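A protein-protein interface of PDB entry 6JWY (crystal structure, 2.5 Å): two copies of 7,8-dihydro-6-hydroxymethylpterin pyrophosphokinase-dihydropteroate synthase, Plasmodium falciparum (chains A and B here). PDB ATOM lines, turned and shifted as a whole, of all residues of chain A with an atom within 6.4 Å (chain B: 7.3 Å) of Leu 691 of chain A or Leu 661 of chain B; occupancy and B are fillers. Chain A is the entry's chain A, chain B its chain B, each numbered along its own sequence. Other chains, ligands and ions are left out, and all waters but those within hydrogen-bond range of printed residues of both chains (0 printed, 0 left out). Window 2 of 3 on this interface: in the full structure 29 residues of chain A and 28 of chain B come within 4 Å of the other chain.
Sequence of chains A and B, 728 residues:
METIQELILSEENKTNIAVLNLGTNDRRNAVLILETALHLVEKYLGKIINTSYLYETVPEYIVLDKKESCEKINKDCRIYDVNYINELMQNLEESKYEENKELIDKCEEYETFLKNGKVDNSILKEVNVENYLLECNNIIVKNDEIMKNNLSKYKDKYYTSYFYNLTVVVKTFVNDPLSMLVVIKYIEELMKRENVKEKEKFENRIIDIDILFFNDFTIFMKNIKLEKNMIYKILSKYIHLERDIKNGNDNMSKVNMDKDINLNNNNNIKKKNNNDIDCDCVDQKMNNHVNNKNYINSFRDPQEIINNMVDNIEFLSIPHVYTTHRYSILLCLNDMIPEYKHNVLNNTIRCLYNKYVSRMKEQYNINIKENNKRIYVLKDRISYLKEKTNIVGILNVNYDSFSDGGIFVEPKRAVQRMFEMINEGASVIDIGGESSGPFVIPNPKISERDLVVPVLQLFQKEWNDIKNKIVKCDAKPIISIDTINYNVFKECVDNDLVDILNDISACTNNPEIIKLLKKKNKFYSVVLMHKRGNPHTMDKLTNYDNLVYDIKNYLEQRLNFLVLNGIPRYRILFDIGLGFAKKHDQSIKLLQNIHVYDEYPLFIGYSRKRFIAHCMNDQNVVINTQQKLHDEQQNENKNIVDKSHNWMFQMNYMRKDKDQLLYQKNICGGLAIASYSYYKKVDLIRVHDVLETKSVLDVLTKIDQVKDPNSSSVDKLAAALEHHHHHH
Of chain B, only Leu 661 comes within 4 Å of Leu 691 of chain A. Of the printed residues of chain A, Leu 661 of chain B touches Leu 691. Of the printed residues of chain A, Met 616 of chain B touches Ser 695 (3.9 Å). Of the printed residues of chain B, Glu 692 of chain A touches Gln 664 and Cys 668. Printed residues of chain A within 4 Å of Cys 668 of chain B: Glu 692, Ser 695 and Val 696. Printed residues of chain A within 4 Å of Gln 664 of chain B: Glu 692. Of the printed residues of chain A, Lys 665 of chain B touches Ser 695. The nearest residue of chain B that does not touch Leu 691 of chain A is Lys 665 of chain B (4.1 Å). The nearest printed residue of chain A that does not touch Leu 661 of chain B is Glu 424 of chain A (6.4 Å).
Of the 13 printed residues of chain B, 5 touch a printed residue of chain A. Printed residues of chain B that touch a printed residue of chain A: Met 616, Leu 661, Gln 664, Lys 665 and Cys 668. Hydrophobic or aromatic side chains of chain B that line the printed part of chain A: Met 616 and Leu 661. Hydrophobic or aromatic side chains of chain A within 4 Å of the printed part of chain B: Leu 691 and Val 696. Among the printed residues, no Asp or Glu carboxylate lies within 4 Å of a Lys or Arg side-chain nitrogen of the other chain.
OE2 of Glu 692 of chain A lies close to OE1 of Gln 664 of chain B, 3.4 Å away.
No position is printed for both chains.
Leu 691 of chain A touches Leu 661 of chain B. Cys 668 of chain B touches Glu 692 of chain A. Ser 695 of chain A touches Met 616 of chain B (CB to SD, 3.9 Å). CG of Lys 665 of chain B touches OG of Ser 695 of chain A, at 3.7 Å. CB of Ser 695 of chain A touches CB of Cys 668 of chain B, 3.6 Å away. O of Cys 668 of chain B touches CG2 of Val 696 of chain A (3.6 Å).
The backbone NH (N) of Leu 691 of chain A sits at hydrogen-bond distance from the side-chain carboxylate (OE1) of Glu 424 of chain A (3.1 Å). O of Leu 691 of chain A lies within hydrogen-bond range of OG of Ser 695 of chain A, 2.8 Å away.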
ATOM      1  N   ILE A 391      24.646  12.465 -16.328  1.00  0.00           N
ATOM      2  CA  ILE A 391      24.018  12.637 -17.623  1.00  0.00           C
ATOM      3  C   ILE A 391      23.798  14.126 -17.844  1.00  0.00           C
ATOM      4  O   ILE A 391      23.221  14.795 -16.983  1.00  0.00           O
ATOM      5  CB  ILE A 391      22.675  11.889 -17.702  1.00  0.00           C
ATOM      6  CG1 ILE A 391      22.861  10.375 -17.607  1.00  0.00           C
ATOM      7  CG2 ILE A 391      21.885  12.322 -18.935  1.00  0.00           C
ATOM      8  CD1 ILE A 391      21.561   9.624 -17.396  1.00  0.00           C
ATOM      9  N   GLU A 424      13.400  12.910 -16.202  1.00  0.00           N
ATOM     10  CA  GLU A 424      13.971  11.735 -16.819  1.00  0.00           C
ATOM     11  C   GLU A 424      15.328  11.432 -16.174  1.00  0.00           C
ATOM     12  O   GLU A 424      15.902  10.361 -16.387  1.00  0.00           O
ATOM     13  CB  GLU A 424      14.049  11.952 -18.327  1.00  0.00           C
ATOM     14  CG  GLU A 424      12.829  11.510 -19.115  1.00  0.00           C
ATOM     15  CD  GLU A 424      12.988  11.635 -20.632  1.00  0.00           C
ATOM     16  OE1 GLU A 424      14.166  11.683 -21.131  1.00  0.00           O
ATOM     17  OE2 GLU A 424      11.935  11.673 -21.342  1.00  0.00           O
ATOM     18  N   GLY A 425      15.863  12.366 -15.382  1.00  0.00           N
ATOM     19  CA  GLY A 425      17.081  12.053 -14.641  1.00  0.00           C
ATOM     20  C   GLY A 425      18.361  12.821 -15.026  1.00  0.00           C
ATOM     21  O   GLY A 425      19.420  12.568 -14.450  1.00  0.00           O
ATOM     22  N   HIS A 688      21.121  12.811 -26.016  1.00  0.00           N
ATOM     23  CA  HIS A 688      19.736  13.107 -26.395  1.00  0.00           C
ATOM     24  C   HIS A 688      18.737  12.284 -25.588  1.00  0.00           C
ATOM     25  O   HIS A 688      17.758  12.834 -25.097  1.00  0.00           O
ATOM     26  CB  HIS A 688      19.466  12.798 -27.876  1.00  0.00           C
ATOM     27  CG  HIS A 688      20.225  13.695 -28.792  1.00  0.00           C
ATOM     28  ND1 HIS A 688      21.427  13.292 -29.384  1.00  0.00           N
ATOM     29  CD2 HIS A 688      19.996  14.974 -29.168  1.00  0.00           C
ATOM     30  CE1 HIS A 688      21.897  14.293 -30.101  1.00  0.00           C
ATOM     31  NE2 HIS A 688      21.031  15.339 -29.982  1.00  0.00           N
ATOM     32  N   ASP A 689      18.975  10.966 -25.492  1.00  0.00           N
ATOM     33  CA  ASP A 689      18.075   9.996 -24.876  1.00  0.00           C
ATOM     34  C   ASP A 689      18.320   9.843 -23.370  1.00  0.00           C
ATOM     35  O   ASP A 689      18.972   8.900 -22.939  1.00  0.00           O
ATOM     36  CB  ASP A 689      18.239   8.683 -25.629  1.00  0.00           C
ATOM     37  CG  ASP A 689      18.106   8.939 -27.126  1.00  0.00           C
ATOM     38  OD1 ASP A 689      17.057   9.496 -27.522  1.00  0.00           O
ATOM     39  OD2 ASP A 689      19.054   8.620 -27.887  1.00  0.00           O
ATOM     40  N   VAL A 690      17.767  10.756 -22.563  1.00  0.00           N
ATOM     41  CA  VAL A 690      18.007  10.815 -21.132  1.00  0.00           C
ATOM     42  C   VAL A 690      17.441   9.581 -20.430  1.00  0.00           C
ATOM     43  O   VAL A 690      18.179   8.834 -19.788  1.00  0.00           O
ATOM     44  CB  VAL A 690      17.477  12.125 -20.522  1.00  0.00           C
ATOM     45  CG1 VAL A 690      17.673  12.189 -19.013  1.00  0.00           C
ATOM     46  CG2 VAL A 690      18.125  13.329 -21.171  1.00  0.00           C
ATOM     47  N   LEU A 691      16.135   9.335 -20.567  1.00  0.00           N
ATOM     48  CA  LEU A 691      15.506   8.245 -19.833  1.00  0.00           C
ATOM     49  C   LEU A 691      16.192   6.913 -20.126  1.00  0.00           C
ATOM     50  O   LEU A 691      16.439   6.148 -19.191  1.00  0.00           O
ATOM     51  CB  LEU A 691      14.008   8.191 -20.162  1.00  0.00           C
ATOM     52  CG  LEU A 691      13.209   7.108 -19.436  1.00  0.00           C
ATOM     53  CD1 LEU A 691      11.831   7.620 -19.068  1.00  0.00           C
ATOM     54  CD2 LEU A 691      13.105   5.855 -20.294  1.00  0.00           C
ATOM     55  N   GLU A 692      16.492   6.628 -21.403  1.00  0.00           N
ATOM     56  CA  GLU A 692      17.119   5.353 -21.726  1.00  0.00           C
ATOM     57  C   GLU A 692      18.510   5.260 -21.106  1.00  0.00           C
ATOM     58  O   GLU A 692      18.873   4.204 -20.571  1.00  0.00           O
ATOM     59  CB  GLU A 692      17.236   5.112 -23.226  1.00  0.00           C
ATOM     60  CG  GLU A 692      15.907   5.154 -23.923  1.00  0.00           C
ATOM     61  CD  GLU A 692      15.385   6.537 -24.260  1.00  0.00           C
ATOM     62  OE1 GLU A 692      15.641   7.520 -23.493  1.00  0.00           O
ATOM     63  OE2 GLU A 692      14.697   6.621 -25.281  1.00  0.00           O
ATOM     64  N   THR A 693      19.272   6.371 -21.190  1.00  0.00           N
ATOM     65  CA  THR A 693      20.617   6.432 -20.629  1.00  0.00           C
ATOM     66  C   THR A 693      20.545   6.228 -19.119  1.00  0.00           C
ATOM     67  O   THR A 693      21.362   5.509 -18.566  1.00  0.00           O
ATOM     68  CB  THR A 693      21.386   7.707 -21.043  1.00  0.00           C
ATOM     69  OG1 THR A 693      21.248   7.925 -22.446  1.00  0.00           O
ATOM     70  CG2 THR A 693      22.859   7.627 -20.719  1.00  0.00           C
ATOM     71  N   LYS A 694      19.578   6.884 -18.465  1.00  0.00           N
ATOM     72  CA  LYS A 694      19.452   6.830 -17.011  1.00  0.00           C
ATOM     73  C   LYS A 694      19.110   5.408 -16.563  1.00  0.00           C
ATOM     74  O   LYS A 694      19.612   4.914 -15.559  1.00  0.00           O
ATOM     75  CB  LYS A 694      18.382   7.795 -16.498  1.00  0.00           C
ATOM     76  CG  LYS A 694      18.220   7.796 -14.985  1.00  0.00           C
ATOM     77  CD  LYS A 694      19.466   8.285 -14.291  1.00  0.00           C
ATOM     78  CE  LYS A 694      19.187   8.961 -12.966  1.00  0.00           C
ATOM     79  NZ  LYS A 694      18.701   7.965 -11.974  1.00  0.00           N
ATOM     80  N   SER A 695      18.259   4.747 -17.336  1.00  0.00           N
ATOM     81  CA  SER A 695      17.863   3.403 -16.971  1.00  0.00           C
ATOM     82  C   SER A 695      19.096   2.506 -16.986  1.00  0.00           C
ATOM     83  O   SER A 695      19.221   1.619 -16.128  1.00  0.00           O
ATOM     84  CB  SER A 695      16.806   2.895 -17.902  1.00  0.00           C
ATOM     85  OG  SER A 695      15.709   3.783 -17.874  1.00  0.00           O
ATOM     86  N   VAL A 696      19.986   2.750 -17.963  1.00  0.00           N
ATOM     87  CA  VAL A 696      21.134   1.873 -18.140  1.00  0.00           C
ATOM     88  C   VAL A 696      22.082   2.066 -16.955  1.00  0.00           C
ATOM     89  O   VAL A 696      22.500   1.090 -16.337  1.00  0.00           O
ATOM     90  CB  VAL A 696      21.830   2.061 -19.503  1.00  0.00           C
ATOM     91  CG1 VAL A 696      23.227   1.469 -19.518  1.00  0.00           C
ATOM     92  CG2 VAL A 696      21.010   1.492 -20.644  1.00  0.00           C
ATOM     93  N   MET B 616      15.514   0.530 -10.204  1.00  0.00           N
ATOM     94  CA  MET B 616      15.397   1.885 -10.717  1.00  0.00           C
ATOM     95  C   MET B 616      14.595   2.766  -9.759  1.00  0.00           C
ATOM     96  O   MET B 616      14.783   3.985  -9.742  1.00  0.00           O
ATOM     97  CB  MET B 616      14.761   1.898 -12.112  1.00  0.00           C
ATOM     98  CG  MET B 616      15.194   0.725 -12.961  1.00  0.00           C
ATOM     99  SD  MET B 616      15.519   1.098 -14.691  1.00  0.00           S
ATOM    100  CE  MET B 616      15.293  -0.511 -15.437  1.00  0.00           C
ATOM    101  N   ASP B 657       0.201   4.631 -19.777  1.00  0.00           N
ATOM    102  CA  ASP B 657       1.364   5.535 -20.002  1.00  0.00           C
ATOM    103  C   ASP B 657       2.429   5.281 -18.939  1.00  0.00           C
ATOM    104  O   ASP B 657       3.568   4.968 -19.272  1.00  0.00           O
ATOM    105  CB  ASP B 657       0.952   7.009 -20.022  1.00  0.00           C
ATOM    106  CG  ASP B 657       2.040   7.938 -20.538  1.00  0.00           C
ATOM    107  OD1 ASP B 657       2.728   7.559 -21.514  1.00  0.00           O
ATOM    108  OD2 ASP B 657       2.193   9.033 -19.960  1.00  0.00           O
ATOM    109  N   LYS B 658       2.046   5.437 -17.664  1.00  0.00           N
ATOM    110  CA  LYS B 658       2.929   5.156 -16.543  1.00  0.00           C
ATOM    111  C   LYS B 658       3.163   3.650 -16.433  1.00  0.00           C
ATOM    112  O   LYS B 658       4.052   3.213 -15.705  1.00  0.00           O
ATOM    113  CB  LYS B 658       2.384   5.768 -15.248  1.00  0.00           C
ATOM    114  CG  LYS B 658       2.561   7.277 -15.114  1.00  0.00           C
ATOM    115  CD  LYS B 658       2.227   7.823 -13.734  1.00  0.00           C
ATOM    116  CE  LYS B 658       3.262   7.492 -12.676  1.00  0.00           C
ATOM    117  NZ  LYS B 658       4.578   8.105 -12.973  1.00  0.00           N
ATOM    118  N   ASP B 659       2.359   2.870 -17.169  1.00  0.00           N
ATOM    119  CA  ASP B 659       2.544   1.432 -17.301  1.00  0.00           C
ATOM    120  C   ASP B 659       3.575   1.155 -18.394  1.00  0.00           C
ATOM    121  O   ASP B 659       4.290   0.152 -18.337  1.00  0.00           O
ATOM    122  CB  ASP B 659       1.224   0.716 -17.617  1.00  0.00           C
ATOM    123  CG  ASP B 659       0.159   0.802 -16.532  1.00  0.00           C
ATOM    124  OD1 ASP B 659       0.523   1.018 -15.354  1.00  0.00           O
ATOM    125  OD2 ASP B 659      -1.034   0.638 -16.874  1.00  0.00           O
ATOM    126  N   GLN B 660       3.636   2.061 -19.382  1.00  0.00           N
ATOM    127  CA  GLN B 660       4.437   1.889 -20.585  1.00  0.00           C
ATOM    128  C   GLN B 660       5.832   2.484 -20.392  1.00  0.00           C
ATOM    129  O   GLN B 660       6.776   2.072 -21.068  1.00  0.00           O
ATOM    130  CB  GLN B 660       3.724   2.485 -21.801  1.00  0.00           C
ATOM    131  CG  GLN B 660       3.991   1.709 -23.087  1.00  0.00           C
ATOM    132  CD  GLN B 660       4.033   2.567 -24.330  1.00  0.00           C
ATOM    133  OE1 GLN B 660       3.535   2.181 -25.388  1.00  0.00           O
ATOM    134  NE2 GLN B 660       4.644   3.738 -24.218  1.00  0.00           N
ATOM    135  N   LEU B 661       5.950   3.448 -19.465  1.00  0.00           N
ATOM    136  CA  LEU B 661       7.237   3.988 -19.055  1.00  0.00           C
ATOM    137  C   LEU B 661       8.074   2.876 -18.436  1.00  0.00           C
ATOM    138  O   LEU B 661       9.251   2.731 -18.757  1.00  0.00           O
ATOM    139  CB  LEU B 661       7.038   5.132 -18.054  1.00  0.00           C
ATOM    140  CG  LEU B 661       6.876   6.520 -18.670  1.00  0.00           C
ATOM    141  CD1 LEU B 661       6.715   7.574 -17.582  1.00  0.00           C
ATOM    142  CD2 LEU B 661       8.055   6.855 -19.573  1.00  0.00           C
ATOM    143  N   LEU B 662       7.436   2.090 -17.564  1.00  0.00           N
ATOM    144  CA  LEU B 662       8.120   1.013 -16.873  1.00  0.00           C
ATOM    145  C   LEU B 662       8.442  -0.110 -17.857  1.00  0.00           C
ATOM    146  O   LEU B 662       9.470  -0.757 -17.710  1.00  0.00           O
ATOM    147  CB  LEU B 662       7.292   0.544 -15.671  1.00  0.00           C
ATOM    148  CG  LEU B 662       6.914   1.619 -14.645  1.00  0.00           C
ATOM    149  CD1 LEU B 662       6.558   0.977 -13.310  1.00  0.00           C
ATOM    150  CD2 LEU B 662       8.021   2.656 -14.448  1.00  0.00           C
ATOM    151  N   TYR B 663       7.597  -0.299 -18.880  1.00  0.00           N
ATOM    152  CA  TYR B 663       7.896  -1.252 -19.942  1.00  0.00           C
ATOM    153  C   TYR B 663       9.194  -0.841 -20.643  1.00  0.00           C
ATOM    154  O   TYR B 663      10.098  -1.664 -20.802  1.00  0.00           O
ATOM    155  CB  TYR B 663       6.701  -1.436 -20.889  1.00  0.00           C
ATOM    156  CG  TYR B 663       6.981  -2.149 -22.194  1.00  0.00           C
ATOM    157  CD1 TYR B 663       7.132  -3.529 -22.249  1.00  0.00           C
ATOM    158  CD2 TYR B 663       7.088  -1.441 -23.387  1.00  0.00           C
ATOM    159  CE1 TYR B 663       7.396  -4.178 -23.450  1.00  0.00           C
ATOM    160  CE2 TYR B 663       7.343  -2.074 -24.596  1.00  0.00           C
ATOM    161  CZ  TYR B 663       7.496  -3.451 -24.629  1.00  0.00           C
ATOM    162  OH  TYR B 663       7.736  -4.072 -25.825  1.00  0.00           O
ATOM    163  N   GLN B 664       9.285   0.440 -21.028  1.00  0.00           N
ATOM    164  CA  GLN B 664      10.449   0.948 -21.736  1.00  0.00           C
ATOM    165  C   GLN B 664      11.685   0.834 -20.845  1.00  0.00           C
ATOM    166  O   GLN B 664      12.685   0.253 -21.265  1.00  0.00           O
ATOM    167  CB  GLN B 664      10.237   2.381 -22.235  1.00  0.00           C
ATOM    168  CG  GLN B 664      11.031   2.684 -23.503  1.00  0.00           C
ATOM    169  CD  GLN B 664      11.130   4.150 -23.864  1.00  0.00           C
ATOM    170  OE1 GLN B 664      12.069   4.590 -24.534  1.00  0.00           O
ATOM    171  NE2 GLN B 664      10.146   4.921 -23.426  1.00  0.00           N
ATOM    172  N   LYS B 665      11.600   1.374 -19.618  1.00  0.00           N
ATOM    173  CA  LYS B 665      12.709   1.342 -18.677  1.00  0.00           C
ATOM    174  C   LYS B 665      13.203  -0.089 -18.495  1.00  0.00           C
ATOM    175  O   LYS B 665      14.385  -0.315 -18.254  1.00  0.00           O
ATOM    176  CB  LYS B 665      12.300   1.856 -17.295  1.00  0.00           C
ATOM    177  CG  LYS B 665      12.081   3.356 -17.186  1.00  0.00           C
ATOM    178  CD  LYS B 665      12.390   3.852 -15.798  1.00  0.00           C
ATOM    179  CE  LYS B 665      11.619   5.112 -15.482  1.00  0.00           C
ATOM    180  NZ  LYS B 665      11.981   5.617 -14.137  1.00  0.00           N
ATOM    181  N   ASN B 666      12.287  -1.050 -18.612  1.00  0.00           N
ATOM    182  CA  ASN B 666      12.649  -2.430 -18.361  1.00  0.00           C
ATOM    183  C   ASN B 666      13.489  -2.960 -19.529  1.00  0.00           C
ATOM    184  O   ASN B 666      14.472  -3.670 -19.314  1.00  0.00           O
ATOM    185  CB  ASN B 666      11.408  -3.246 -17.989  1.00  0.00           C
ATOM    186  CG  ASN B 666      11.723  -4.584 -17.368  1.00  0.00           C
ATOM    187  OD1 ASN B 666      11.588  -4.749 -16.154  1.00  0.00           O
ATOM    188  ND2 ASN B 666      12.151  -5.535 -18.187  1.00  0.00           N
ATOM    189  N   ILE B 667      13.109  -2.613 -20.766  1.00  0.00           N
ATOM    190  CA  ILE B 667      13.915  -2.990 -21.914  1.00  0.00           C
ATOM    191  C   ILE B 667      15.285  -2.312 -21.821  1.00  0.00           C
ATOM    192  O   ILE B 667      16.316  -2.913 -22.136  1.00  0.00           O
ATOM    193  CB  ILE B 667      13.213  -2.610 -23.222  1.00  0.00           C
ATOM    194  CG1 ILE B 667      11.700  -2.858 -23.154  1.00  0.00           C
ATOM    195  CG2 ILE B 667      13.893  -3.334 -24.382  1.00  0.00           C
ATOM    196  CD1 ILE B 667      11.210  -4.069 -23.942  1.00  0.00           C
ATOM    197  N   CYS B 668      15.284  -1.053 -21.372  1.00  0.00           N
ATOM    198  CA  CYS B 668      16.504  -0.276 -21.296  1.00  0.00           C
ATOM    199  C   CYS B 668      17.428  -0.899 -20.257  1.00  0.00           C
ATOM    200  O   CYS B 668      18.588  -1.186 -20.556  1.00  0.00           O
ATOM    201  CB  CYS B 668      16.191   1.193 -21.029  1.00  0.00           C
ATOM    202  SG  CYS B 668      15.657   2.057 -22.534  1.00  0.00           S
